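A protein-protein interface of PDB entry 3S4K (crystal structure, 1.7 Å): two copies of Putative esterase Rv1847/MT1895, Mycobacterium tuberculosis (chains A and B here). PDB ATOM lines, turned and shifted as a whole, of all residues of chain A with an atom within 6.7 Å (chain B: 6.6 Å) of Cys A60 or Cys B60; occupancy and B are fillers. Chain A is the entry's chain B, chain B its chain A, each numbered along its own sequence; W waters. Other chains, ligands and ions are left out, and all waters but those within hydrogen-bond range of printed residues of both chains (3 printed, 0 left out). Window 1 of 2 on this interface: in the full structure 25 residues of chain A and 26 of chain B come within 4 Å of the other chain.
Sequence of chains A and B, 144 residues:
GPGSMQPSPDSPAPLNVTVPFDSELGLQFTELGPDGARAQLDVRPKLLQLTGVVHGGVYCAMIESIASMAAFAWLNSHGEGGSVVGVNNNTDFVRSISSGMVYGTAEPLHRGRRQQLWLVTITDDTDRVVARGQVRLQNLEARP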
ATOM      1  N   HIS A  55      15.058 -18.292  15.824  1.00  0.00           N
ATOM      2  CA  HIS A  55      14.346 -19.017  14.770  1.00  0.00           C
ATOM      3  C   HIS A  55      12.955 -18.426  14.588  1.00  0.00           C
ATOM      4  O   HIS A  55      12.214 -18.265  15.555  1.00  0.00           O
ATOM      5  CB  HIS A  55      14.271 -20.478  15.165  1.00  0.00           C
ATOM      6  CG  HIS A  55      13.805 -21.390  14.080  1.00  0.00           C
ATOM      7  ND1 HIS A  55      12.510 -21.394  13.619  1.00  0.00           N
ATOM      8  CD2 HIS A  55      14.445 -22.387  13.422  1.00  0.00           C
ATOM      9  CE1 HIS A  55      12.378 -22.333  12.698  1.00  0.00           C
ATOM     10  NE2 HIS A  55      13.536 -22.950  12.561  1.00  0.00           N
ATOM     11  N   GLY A  56      12.606 -18.048  13.358  1.00  0.00           N
ATOM     12  CA  GLY A  56      11.286 -17.448  13.097  1.00  0.00           C
ATOM     13  C   GLY A  56      10.087 -18.229  13.622  1.00  0.00           C
ATOM     14  O   GLY A  56       9.059 -17.661  14.045  1.00  0.00           O
ATOM     15  N   GLY A  57      10.206 -19.539  13.551  1.00  0.00           N
ATOM     16  CA  GLY A  57       9.222 -20.460  14.125  1.00  0.00           C
ATOM     17  C   GLY A  57       8.879 -20.190  15.572  1.00  0.00           C
ATOM     18  O   GLY A  57       7.742 -20.408  15.983  1.00  0.00           O
ATOM     19  N   VAL A  58       9.855 -19.736  16.365  1.00  0.00           N
ATOM     20  CA  VAL A  58       9.596 -19.396  17.772  1.00  0.00           C
ATOM     21  C   VAL A  58       8.548 -18.296  17.870  1.00  0.00           C
ATOM     22  O   VAL A  58       7.592 -18.387  18.623  1.00  0.00           O
ATOM     23  CB  VAL A  58      10.885 -18.941  18.463  1.00  0.00           C
ATOM     24  CG1 VAL A  58      10.603 -18.361  19.875  1.00  0.00           C
ATOM     25  CG2 VAL A  58      11.893 -20.117  18.507  1.00  0.00           C
ATOM     26  N   TYR A  59       8.715 -17.263  17.056  1.00  0.00           N
ATOM     27  CA  TYR A  59       7.747 -16.169  17.026  1.00  0.00           C
ATOM     28  C   TYR A  59       6.403 -16.606  16.459  1.00  0.00           C
ATOM     29  O   TYR A  59       5.357 -16.232  17.001  1.00  0.00           O
ATOM     30  CB  TYR A  59       8.256 -14.999  16.199  1.00  0.00           C
ATOM     31  CG  TYR A  59       9.502 -14.341  16.736  1.00  0.00           C
ATOM     32  CD1 TYR A  59       9.591 -13.968  18.066  1.00  0.00           C
ATOM     33  CD2 TYR A  59      10.553 -14.011  15.888  1.00  0.00           C
ATOM     34  CE1 TYR A  59      10.734 -13.333  18.565  1.00  0.00           C
ATOM     35  CE2 TYR A  59      11.719 -13.379  16.368  1.00  0.00           C
ATOM     36  CZ  TYR A  59      11.804 -13.042  17.692  1.00  0.00           C
ATOM     37  OH  TYR A  59      12.949 -12.418  18.133  1.00  0.00           O
ATOM     38  N   CYS A  60       6.402 -17.355  15.356  1.00  0.00           N
ATOM     39  CA  CYS A  60       5.134 -17.919  14.878  1.00  0.00           C
ATOM     40  C   CYS A  60       4.380 -18.639  15.997  1.00  0.00           C
ATOM     41  O   CYS A  60       3.173 -18.512  16.134  1.00  0.00           O
ATOM     42  CB  CYS A  60       5.382 -18.879  13.741  1.00  0.00           C
ATOM     43  SG  CYS A  60       6.113 -18.157  12.255  1.00  0.00           S
ATOM     44  N   ALA A  61       5.122 -19.403  16.795  1.00  0.00           N
ATOM     45  CA  ALA A  61       4.532 -20.216  17.850  1.00  0.00           C
ATOM     46  C   ALA A  61       3.997 -19.374  18.993  1.00  0.00           C
ATOM     47  O   ALA A  61       2.889 -19.587  19.509  1.00  0.00           O
ATOM     48  CB  ALA A  61       5.552 -21.230  18.382  1.00  0.00           C
ATOM     49  N   MET A  62       4.782 -18.392  19.378  1.00  0.00           N
ATOM     50  CA  MET A  62       4.388 -17.417  20.386  1.00  0.00           C
ATOM     51  C   MET A  62       3.093 -16.698  19.979  1.00  0.00           C
ATOM     52  O   MET A  62       2.141 -16.559  20.765  1.00  0.00           O
ATOM     53  CB  MET A  62       5.536 -16.418  20.519  1.00  0.00           C
ATOM     54  CG  MET A  62       5.417 -15.404  21.607  1.00  0.00           C
ATOM     55  SD  MET A  62       7.087 -14.821  22.004  1.00  0.00           S
ATOM     56  CE  MET A  62       6.651 -13.591  23.258  1.00  0.00           C
ATOM     57  N   ILE A  63       3.074 -16.231  18.745  1.00  0.00           N
ATOM     58  CA  ILE A  63       1.904 -15.587  18.174  1.00  0.00           C
ATOM     59  C   ILE A  63       0.698 -16.517  18.211  1.00  0.00           C
ATOM     60  O   ILE A  63      -0.376 -16.127  18.645  1.00  0.00           O
ATOM     61  CB  ILE A  63       2.250 -15.060  16.766  1.00  0.00           C
ATOM     62  CG1 ILE A  63       3.109 -13.805  16.892  1.00  0.00           C
ATOM     63  CG2 ILE A  63       1.001 -14.810  15.918  1.00  0.00           C
ATOM     64  CD1 ILE A  63       3.932 -13.479  15.647  1.00  0.00           C
ATOM     65  N   GLU A  64       0.884 -17.776  17.819  1.00  0.00           N
ATOM     66  CA  GLU A  64      -0.209 -18.735  17.822  1.00  0.00           C
ATOM     67  C   GLU A  64      -0.779 -18.969  19.220  1.00  0.00           C
ATOM     68  O   GLU A  64      -1.998 -18.951  19.418  1.00  0.00           O
ATOM     69  CB  GLU A  64       0.275 -20.058  17.193  1.00  0.00           C
ATOM     70  CG  GLU A  64      -0.790 -21.118  17.020  1.00  0.00           C
ATOM     71  CD  GLU A  64      -1.756 -20.843  15.872  1.00  0.00           C
ATOM     72  OE1 GLU A  64      -1.521 -19.924  15.076  1.00  0.00           O
ATOM     73  OE2 GLU A  64      -2.772 -21.566  15.762  1.00  0.00           O
ATOM     74  N   SER A  65       0.102 -19.163  20.197  1.00  0.00           N
ATOM     75  CA  SER A  65      -0.292 -19.392  21.586  1.00  0.00           C
ATOM     76  C   SER A  65      -1.060 -18.224  22.172  1.00  0.00           C
ATOM     77  O   SER A  65      -2.143 -18.382  22.751  1.00  0.00           O
ATOM     78  CB  SER A  65       0.942 -19.623  22.461  1.00  0.00           C
ATOM     79  OG  SER A  65       1.330 -20.975  22.430  1.00  0.00           O
ATOM     80  N   ASN A  89      -2.128 -18.587  10.259  1.00  0.00           N
ATOM     81  CA  ASN A  89      -1.187 -17.798  11.031  1.00  0.00           C
ATOM     82  C   ASN A  89      -0.260 -17.126  10.032  1.00  0.00           C
ATOM     83  O   ASN A  89       0.455 -17.807   9.275  1.00  0.00           O
ATOM     84  CB  ASN A  89      -0.387 -18.684  11.998  1.00  0.00           C
ATOM     85  CG  ASN A  89       0.700 -17.916  12.766  1.00  0.00           C
ATOM     86  OD1 ASN A  89       1.446 -17.090  12.218  1.00  0.00           O
ATOM     87  ND2 ASN A  89       0.843 -18.249  14.049  1.00  0.00           N
ATOM     88  N   THR A  91       2.633 -14.382   9.839  1.00  0.00           N
ATOM     89  CA  THR A  91       3.599 -13.695  10.685  1.00  0.00           C
ATOM     90  C   THR A  91       4.629 -12.966   9.827  1.00  0.00           C
ATOM     91  O   THR A  91       5.201 -13.542   8.879  1.00  0.00           O
ATOM     92  CB  THR A  91       4.315 -14.692  11.634  1.00  0.00           C
ATOM     93  OG1 THR A  91       3.376 -15.170  12.597  1.00  0.00           O
ATOM     94  CG2 THR A  91       5.458 -14.027  12.339  1.00  0.00           C
ATOM     95  N   PHE A  93       8.256 -11.065  10.000  1.00  0.00           N
ATOM     96  CA  PHE A  93       9.478 -10.969  10.767  1.00  0.00           C
ATOM     97  C   PHE A  93      10.098  -9.596  10.524  1.00  0.00           C
ATOM     98  O   PHE A  93      10.301  -9.174   9.384  1.00  0.00           O
ATOM     99  CB  PHE A  93      10.425 -12.069  10.344  1.00  0.00           C
ATOM    100  CG  PHE A  93       9.829 -13.450  10.453  1.00  0.00           C
ATOM    101  CD1 PHE A  93       9.398 -13.952  11.683  1.00  0.00           C
ATOM    102  CD2 PHE A  93       9.682 -14.237   9.327  1.00  0.00           C
ATOM    103  CE1 PHE A  93       8.844 -15.217  11.787  1.00  0.00           C
ATOM    104  CE2 PHE A  93       9.139 -15.509   9.430  1.00  0.00           C
ATOM    105  CZ  PHE A  93       8.716 -16.004  10.649  1.00  0.00           C
ATOM    106  N   ILE A 122       5.162  -8.743  18.887  1.00  0.00           N
ATOM    107  CA  ILE A 122       6.262  -9.148  19.763  1.00  0.00           C
ATOM    108  C   ILE A 122       7.341  -8.072  19.769  1.00  0.00           C
ATOM    109  O   ILE A 122       7.822  -7.662  18.712  1.00  0.00           O
ATOM    110  CB  ILE A 122       6.910 -10.449  19.297  1.00  0.00           C
ATOM    111  CG1 ILE A 122       5.811 -11.494  18.988  1.00  0.00           C
ATOM    112  CG2 ILE A 122       7.892 -10.895  20.337  1.00  0.00           C
ATOM    113  CD1 ILE A 122       6.285 -12.943  19.010  1.00  0.00           C
ATOM    114  N   ALA A 131       8.674  -9.210  15.655  1.00  0.00           N
ATOM    115  CA  ALA A 131       7.729  -9.959  14.805  1.00  0.00           C
ATOM    116  C   ALA A 131       6.301  -9.506  15.103  1.00  0.00           C
ATOM    117  O   ALA A 131       6.015  -8.982  16.179  1.00  0.00           O
ATOM    118  CB  ALA A 131       7.892 -11.516  14.965  1.00  0.00           C
ATOM    119  N   VAL A 135      -3.663 -14.206  13.525  1.00  0.00           N
ATOM    120  CA  VAL A 135      -4.125 -15.571  13.614  1.00  0.00           C
ATOM    121  C   VAL A 135      -5.614 -15.591  13.421  1.00  0.00           C
ATOM    122  O   VAL A 135      -6.338 -14.892  14.136  1.00  0.00           O
ATOM    123  CB  VAL A 135      -3.780 -16.199  14.988  1.00  0.00           C
ATOM    124  CG1 VAL A 135      -4.204 -17.683  15.013  1.00  0.00           C
ATOM    125  CG2 VAL A 135      -2.246 -16.028  15.295  1.00  0.00           C
ATOM    126  N   HIS B  55       0.625 -28.448  18.407  1.00  0.00           N
ATOM    127  CA  HIS B  55       0.645 -26.971  18.466  1.00  0.00           C
ATOM    128  C   HIS B  55       0.935 -26.423  17.071  1.00  0.00           C
ATOM    129  O   HIS B  55       1.904 -26.827  16.414  1.00  0.00           O
ATOM    130  CB  HIS B  55       1.724 -26.542  19.443  1.00  0.00           C
ATOM    131  CG  HIS B  55       1.700 -25.094  19.817  1.00  0.00           C
ATOM    132  ND1 HIS B  55       1.951 -24.085  18.915  1.00  0.00           N
ATOM    133  CD2 HIS B  55       1.533 -24.490  21.021  1.00  0.00           C
ATOM    134  CE1 HIS B  55       1.919 -22.920  19.540  1.00  0.00           C
ATOM    135  NE2 HIS B  55       1.664 -23.139  20.818  1.00  0.00           N
ATOM    136  N   GLY B  56       0.069 -25.546  16.578  1.00  0.00           N
ATOM    137  CA  GLY B  56       0.244 -24.996  15.234  1.00  0.00           C
ATOM    138  C   GLY B  56       1.619 -24.397  14.977  1.00  0.00           C
ATOM    139  O   GLY B  56       2.165 -24.462  13.852  1.00  0.00           O
ATOM    140  N   GLY B  57       2.169 -23.788  16.016  1.00  0.00           N
ATOM    141  CA  GLY B  57       3.542 -23.280  16.002  1.00  0.00           C
ATOM    142  C   GLY B  57       4.587 -24.264  15.528  1.00  0.00           C
ATOM    143  O   GLY B  57       5.596 -23.865  14.949  1.00  0.00           O
ATOM    144  N   VAL B  58       4.383 -25.551  15.818  1.00  0.00           N
ATOM    145  CA  VAL B  58       5.314 -26.606  15.381  1.00  0.00           C
ATOM    146  C   VAL B  58       5.374 -26.677  13.866  1.00  0.00           C
ATOM    147  O   VAL B  58       6.460 -26.689  13.269  1.00  0.00           O
ATOM    148  CB  VAL B  58       4.886 -27.974  15.959  1.00  0.00           C
ATOM    149  CG1 VAL B  58       5.633 -29.166  15.315  1.00  0.00           C
ATOM    150  CG2 VAL B  58       5.037 -27.965  17.472  1.00  0.00           C
ATOM    151  N   TYR B  59       4.198 -26.675  13.247  1.00  0.00           N
ATOM    152  CA  TYR B  59       4.093 -26.647  11.789  1.00  0.00           C
ATOM    153  C   TYR B  59       4.645 -25.352  11.200  1.00  0.00           C
ATOM    154  O   TYR B  59       5.386 -25.393  10.223  1.00  0.00           O
ATOM    155  CB  TYR B  59       2.651 -26.829  11.317  1.00  0.00           C
ATOM    156  CG  TYR B  59       2.040 -28.165  11.686  1.00  0.00           C
ATOM    157  CD1 TYR B  59       2.710 -29.349  11.446  1.00  0.00           C
ATOM    158  CD2 TYR B  59       0.762 -28.237  12.216  1.00  0.00           C
ATOM    159  CE1 TYR B  59       2.151 -30.577  11.782  1.00  0.00           C
ATOM    160  CE2 TYR B  59       0.183 -29.459  12.550  1.00  0.00           C
ATOM    161  CZ  TYR B  59       0.868 -30.616  12.326  1.00  0.00           C
ATOM    162  OH  TYR B  59       0.282 -31.820  12.646  1.00  0.00           O
ATOM    163  N   CYS B  60       4.256 -24.213  11.757  1.00  0.00           N
ATOM    164  CA  CYS B  60       4.906 -22.953  11.370  1.00  0.00           C
ATOM    165  C   CYS B  60       6.428 -23.046  11.347  1.00  0.00           C
ATOM    166  O   CYS B  60       7.075 -22.615  10.407  1.00  0.00           O
ATOM    167  CB  CYS B  60       4.480 -21.847  12.295  1.00  0.00           C
ATOM    168  SG  CYS B  60       2.742 -21.426  12.204  1.00  0.00           S
ATOM    169  N   ALA B  61       6.998 -23.623  12.398  1.00  0.00           N
ATOM    170  CA  ALA B  61       8.436 -23.706  12.537  1.00  0.00           C
ATOM    171  C   ALA B  61       9.076 -24.653  11.531  1.00  0.00           C
ATOM    172  O   ALA B  61      10.120 -24.374  10.934  1.00  0.00           O
ATOM    173  CB  ALA B  61       8.786 -24.132  13.988  1.00  0.00           C
ATOM    174  N   MET B  62       8.429 -25.793  11.346  1.00  0.00           N
ATOM    175  CA  MET B  62       8.830 -26.790  10.343  1.00  0.00           C
ATOM    176  C   MET B  62       8.882 -26.161   8.961  1.00  0.00           C
ATOM    177  O   MET B  62       9.864 -26.297   8.210  1.00  0.00           O
ATOM    178  CB  MET B  62       7.814 -27.932  10.272  1.00  0.00           C
ATOM    179  CG  MET B  62       8.033 -29.089  11.208  1.00  0.00           C
ATOM    180  SD  MET B  62       6.999 -30.481  10.663  1.00  0.00           S
ATOM    181  CE  MET B  62       7.886 -31.125   9.248  1.00  0.00           C
ATOM    182  N   ILE B  63       7.809 -25.465   8.624  1.00  0.00           N
ATOM    183  CA  ILE B  63       7.669 -24.788   7.342  1.00  0.00           C
ATOM    184  C   ILE B  63       8.784 -23.757   7.202  1.00  0.00           C
ATOM    185  O   ILE B  63       9.438 -23.683   6.178  1.00  0.00           O
ATOM    186  CB  ILE B  63       6.234 -24.201   7.217  1.00  0.00           C
ATOM    187  CG1 ILE B  63       5.258 -25.335   6.921  1.00  0.00           C
ATOM    188  CG2 ILE B  63       6.135 -23.037   6.162  1.00  0.00           C
ATOM    189  CD1 ILE B  63       3.823 -25.033   7.297  1.00  0.00           C
ATOM    190  N   GLU B  64       9.053 -23.012   8.264  1.00  0.00           N
ATOM    191  CA  GLU B  64      10.109 -21.991   8.226  1.00  0.00           C
ATOM    192  C   GLU B  64      11.490 -22.596   7.956  1.00  0.00           C
ATOM    193  O   GLU B  64      12.246 -22.109   7.094  1.00  0.00           O
ATOM    194  CB  GLU B  64      10.094 -21.202   9.543  1.00  0.00           C
ATOM    195  CG  GLU B  64      11.090 -20.037   9.605  1.00  0.00           C
ATOM    196  CD  GLU B  64      10.675 -18.831   8.793  1.00  0.00           C
ATOM    197  OE1 GLU B  64       9.533 -18.800   8.278  1.00  0.00           O
ATOM    198  OE2 GLU B  64      11.513 -17.895   8.676  1.00  0.00           O
ATOM    199  N   SER B  65      11.808 -23.676   8.672  1.00  0.00           N
ATOM    200  CA  SER B  65      13.093 -24.357   8.542  1.00  0.00           C
ATOM    201  C   SER B  65      13.309 -24.942   7.153  1.00  0.00           C
ATOM    202  O   SER B  65      14.354 -24.755   6.532  1.00  0.00           O
ATOM    203  CB  SER B  65      13.210 -25.491   9.568  1.00  0.00           C
ATOM    204  OG  SER B  65      13.533 -24.986  10.847  1.00  0.00           O
ATOM    205  N   ASN B  89       5.854 -15.565   6.926  1.00  0.00           N
ATOM    206  CA  ASN B  89       5.489 -16.987   6.999  1.00  0.00           C
ATOM    207  C   ASN B  89       3.979 -17.052   7.161  1.00  0.00           C
ATOM    208  O   ASN B  89       3.424 -16.530   8.163  1.00  0.00           O
ATOM    209  CB  ASN B  89       6.200 -17.694   8.171  1.00  0.00           C
ATOM    210  CG  ASN B  89       5.768 -19.168   8.362  1.00  0.00           C
ATOM    211  OD1 ASN B  89       4.569 -19.518   8.343  1.00  0.00           O
ATOM    212  ND2 ASN B  89       6.766 -20.030   8.654  1.00  0.00           N
ATOM    213  N   THR B  91       0.955 -19.688   7.117  1.00  0.00           N
ATOM    214  CA  THR B  91       0.671 -21.108   7.259  1.00  0.00           C
ATOM    215  C   THR B  91      -0.804 -21.336   7.472  1.00  0.00           C
ATOM    216  O   THR B  91      -1.441 -20.672   8.308  1.00  0.00           O
ATOM    217  CB  THR B  91       1.424 -21.705   8.460  1.00  0.00           C
ATOM    218  OG1 THR B  91       2.816 -21.641   8.186  1.00  0.00           O
ATOM    219  CG2 THR B  91       0.994 -23.138   8.645  1.00  0.00           C
ATOM    220  N   PHE B  93      -3.535 -24.201   8.590  1.00  0.00           N
ATOM    221  CA  PHE B  93      -3.685 -25.427   9.338  1.00  0.00           C
ATOM    222  C   PHE B  93      -4.883 -26.176   8.784  1.00  0.00           C
ATOM    223  O   PHE B  93      -5.969 -25.614   8.645  1.00  0.00           O
ATOM    224  CB  PHE B  93      -3.901 -25.098  10.808  1.00  0.00           C
ATOM    225  CG  PHE B  93      -2.838 -24.212  11.390  1.00  0.00           C
ATOM    226  CD1 PHE B  93      -1.504 -24.626  11.433  1.00  0.00           C
ATOM    227  CD2 PHE B  93      -3.160 -22.959  11.877  1.00  0.00           C
ATOM    228  CE1 PHE B  93      -0.529 -23.822  11.975  1.00  0.00           C
ATOM    229  CE2 PHE B  93      -2.177 -22.145  12.425  1.00  0.00           C
ATOM    230  CZ  PHE B  93      -0.848 -22.577  12.461  1.00  0.00           C
ATOM    231  N   ILE B 122       2.982 -30.087   4.604  1.00  0.00           N
ATOM    232  CA  ILE B 122       3.218 -31.082   5.650  1.00  0.00           C
ATOM    233  C   ILE B 122       2.129 -32.141   5.613  1.00  0.00           C
ATOM    234  O   ILE B 122       0.944 -31.812   5.670  1.00  0.00           O
ATOM    235  CB  ILE B 122       3.210 -30.449   7.049  1.00  0.00           C
ATOM    236  CG1 ILE B 122       4.076 -29.185   7.063  1.00  0.00           C
ATOM    237  CG2 ILE B 122       3.701 -31.444   8.062  1.00  0.00           C
ATOM    238  CD1 ILE B 122       4.606 -28.834   8.445  1.00  0.00           C
ATOM    239  N   ALA B 131      -0.786 -29.319   7.404  1.00  0.00           N
ATOM    240  CA  ALA B 131      -0.511 -27.880   7.325  1.00  0.00           C
ATOM    241  C   ALA B 131       0.186 -27.581   6.000  1.00  0.00           C
ATOM    242  O   ALA B 131       0.830 -28.474   5.416  1.00  0.00           O
ATOM    243  CB  ALA B 131       0.344 -27.414   8.524  1.00  0.00           C
ATOM    244  N   VAL B 135       6.664 -19.236   2.633  1.00  0.00           N
ATOM    245  CA  VAL B 135       7.659 -18.428   3.289  1.00  0.00           C
ATOM    246  C   VAL B 135       8.327 -17.501   2.287  1.00  0.00           C
ATOM    247  O   VAL B 135       8.830 -17.961   1.258  1.00  0.00           O
ATOM    248  CB  VAL B 135       8.704 -19.328   3.973  1.00  0.00           C
ATOM    249  CG1 VAL B 135       9.748 -18.488   4.722  1.00  0.00           C
ATOM    250  CG2 VAL B 135       8.013 -20.317   4.906  1.00  0.00           C
HETATM  251  O   HOH W   1      14.143 -18.473  10.597  1.00  0.00           O
HETATM  252  O   HOH W   2       3.173 -18.556  10.437  1.00  0.00           O
HETATM  253  O   HOH W   3      -2.354 -24.164  18.067  1.00  0.00           O
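NE2 of His B55 is in hydrogen-bond range of OG of Ser A65 (2.7 Å). OG of Ser B65 is in hydrogen-bond range of NE2 of His A55, at 2.7 Å. The backbone NH (N) of Thr A91 is in hydrogen-bond range of the backbone carbonyl oxygen (O) of Asn B89 (2.8 Å). N of Thr B91 sits at hydrogen-bond distance from O of Asn A89 (2.9 Å). The backbone carbonyl oxygen (O) of Asn A89 lies close to the backbone carbonyl oxygen (O) of Asn B89 (3.4 Å).
The backbone NH (N) of Gly B57 sits at hydrogen-bond distance from a ring nitrogen (ND1) of His B55, 2.9 Å away. O of Gly B56 sits at hydrogen-bond distance from SG of Cys B60 (3.5 Å). OG of Ser B65 sits at hydrogen-bond distance from O of Ala B61, at 3.5 Å. OD1 of Asn B89 sits at hydrogen-bond distance from OG1 of Thr B91 (2.8 Å). ND1 of His A55 is in hydrogen-bond range of N of Gly A57 (3.0 Å). The backbone carbonyl oxygen (O) of Gly A56 lies within hydrogen-bond range of the side-chain sulfur (SG) of Cys A60 (3.5 Å).
Among the printed residues, merely in contact across the chains: His A55 with Ala B61 (3.5 Å), Gly A57 with Ala B61 (3.7 Å), Cys A60 with Cys B60 (3.4 Å), Ala A61 with His B55 (3.5 Å), Ala A61 with Gly B57 (3.7 Å), Glu A64 with Phe B93 (3.4 Å), Asn A89 with Phe B93 (3.9 Å), Phe A93 with Glu B64 (3.4 Å) and Phe A93 with Asn B89 (3.9 Å).
Cys A60 touches one residue of chain B. Cys B60 touches just one residue of chain A: Cys A60 (3.4 Å). Of the printed residues of chain A, Asn B89 touches Asn A89, Thr A91 and Phe A93. Printed residues of chain A within 4 Å of Phe B93: Glu A64 and Asn A89. Printed residues of chain A within 4 Å of Ala B61: His A55 (3.5 Å) and Gly A57 (3.7 Å). Of the printed residues of chain A, Glu B64 touches Phe A93 (3.4 Å). The nearest residue of chain B that does not touch Cys A60 is Asn B89 (4.04 Å). The nearest residue of chain A that does not touch Cys B60 is Asn A89 (4.1 Å). The nearest printed residue of chain A that does not touch Asn B89 is Cys A60 (4.04 Å).
Printed residues of chain A that touch a printed residue of chain B: His A55, Gly A57, Cys A60, Ala A61, Glu A64, Ser A65, Asn A89, Thr A91 and Phe A93. Hydrophobic or aromatic side chains of chain A within 4 Å of the printed part of chain B: His A55, Ala A61 and Phe A93. Printed residues of chain B that touch a printed residue of chain A: His B55, Gly B57, Cys B60, Ala B61, Glu B64, Ser B65, Asn B89, Thr B91 and Phe B93. Hydrophobic or aromatic side chains of chain B within 4 Å of the printed part of chain A: His B55, Ala B61 and Phe B93. Among the printed residues, no Asp or Glu carboxylate lies within 4 Å of a Lys or Arg side-chain nitrogen of the other chain.
His A55 touches Ser B65, and with the chains exchanged Ser A65 touches His B55. Glu A64 touches Phe B93, and with the chains exchanged Phe A93 touches Glu B64. Asn A89 touches its own counterpart, Asn B89. Asn A89 touches Thr B91, and with the chains exchanged Thr A91 touches Asn B89. Positions printed for both chains: 55, 56, 57, 58, 59, 60, 61, 62, 63, 64, 65, 89, 91, 93, 122, 131 and 135.
Water W2 lies within hydrogen-bond range of OD1 of Asn B89, OD1 of Asn A89, SG of Cys B60 and SG of Cys A60. Water W3 bridges the backbone NH of Gly B56 (3.2 Å) and the side-chain carboxylate of Glu A64 (3.5 Å). Water W1 lies within hydrogen-bond range of the backbone NH (N) of Gly A56 and the side-chain carboxylate (OE2) of Glu B64.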
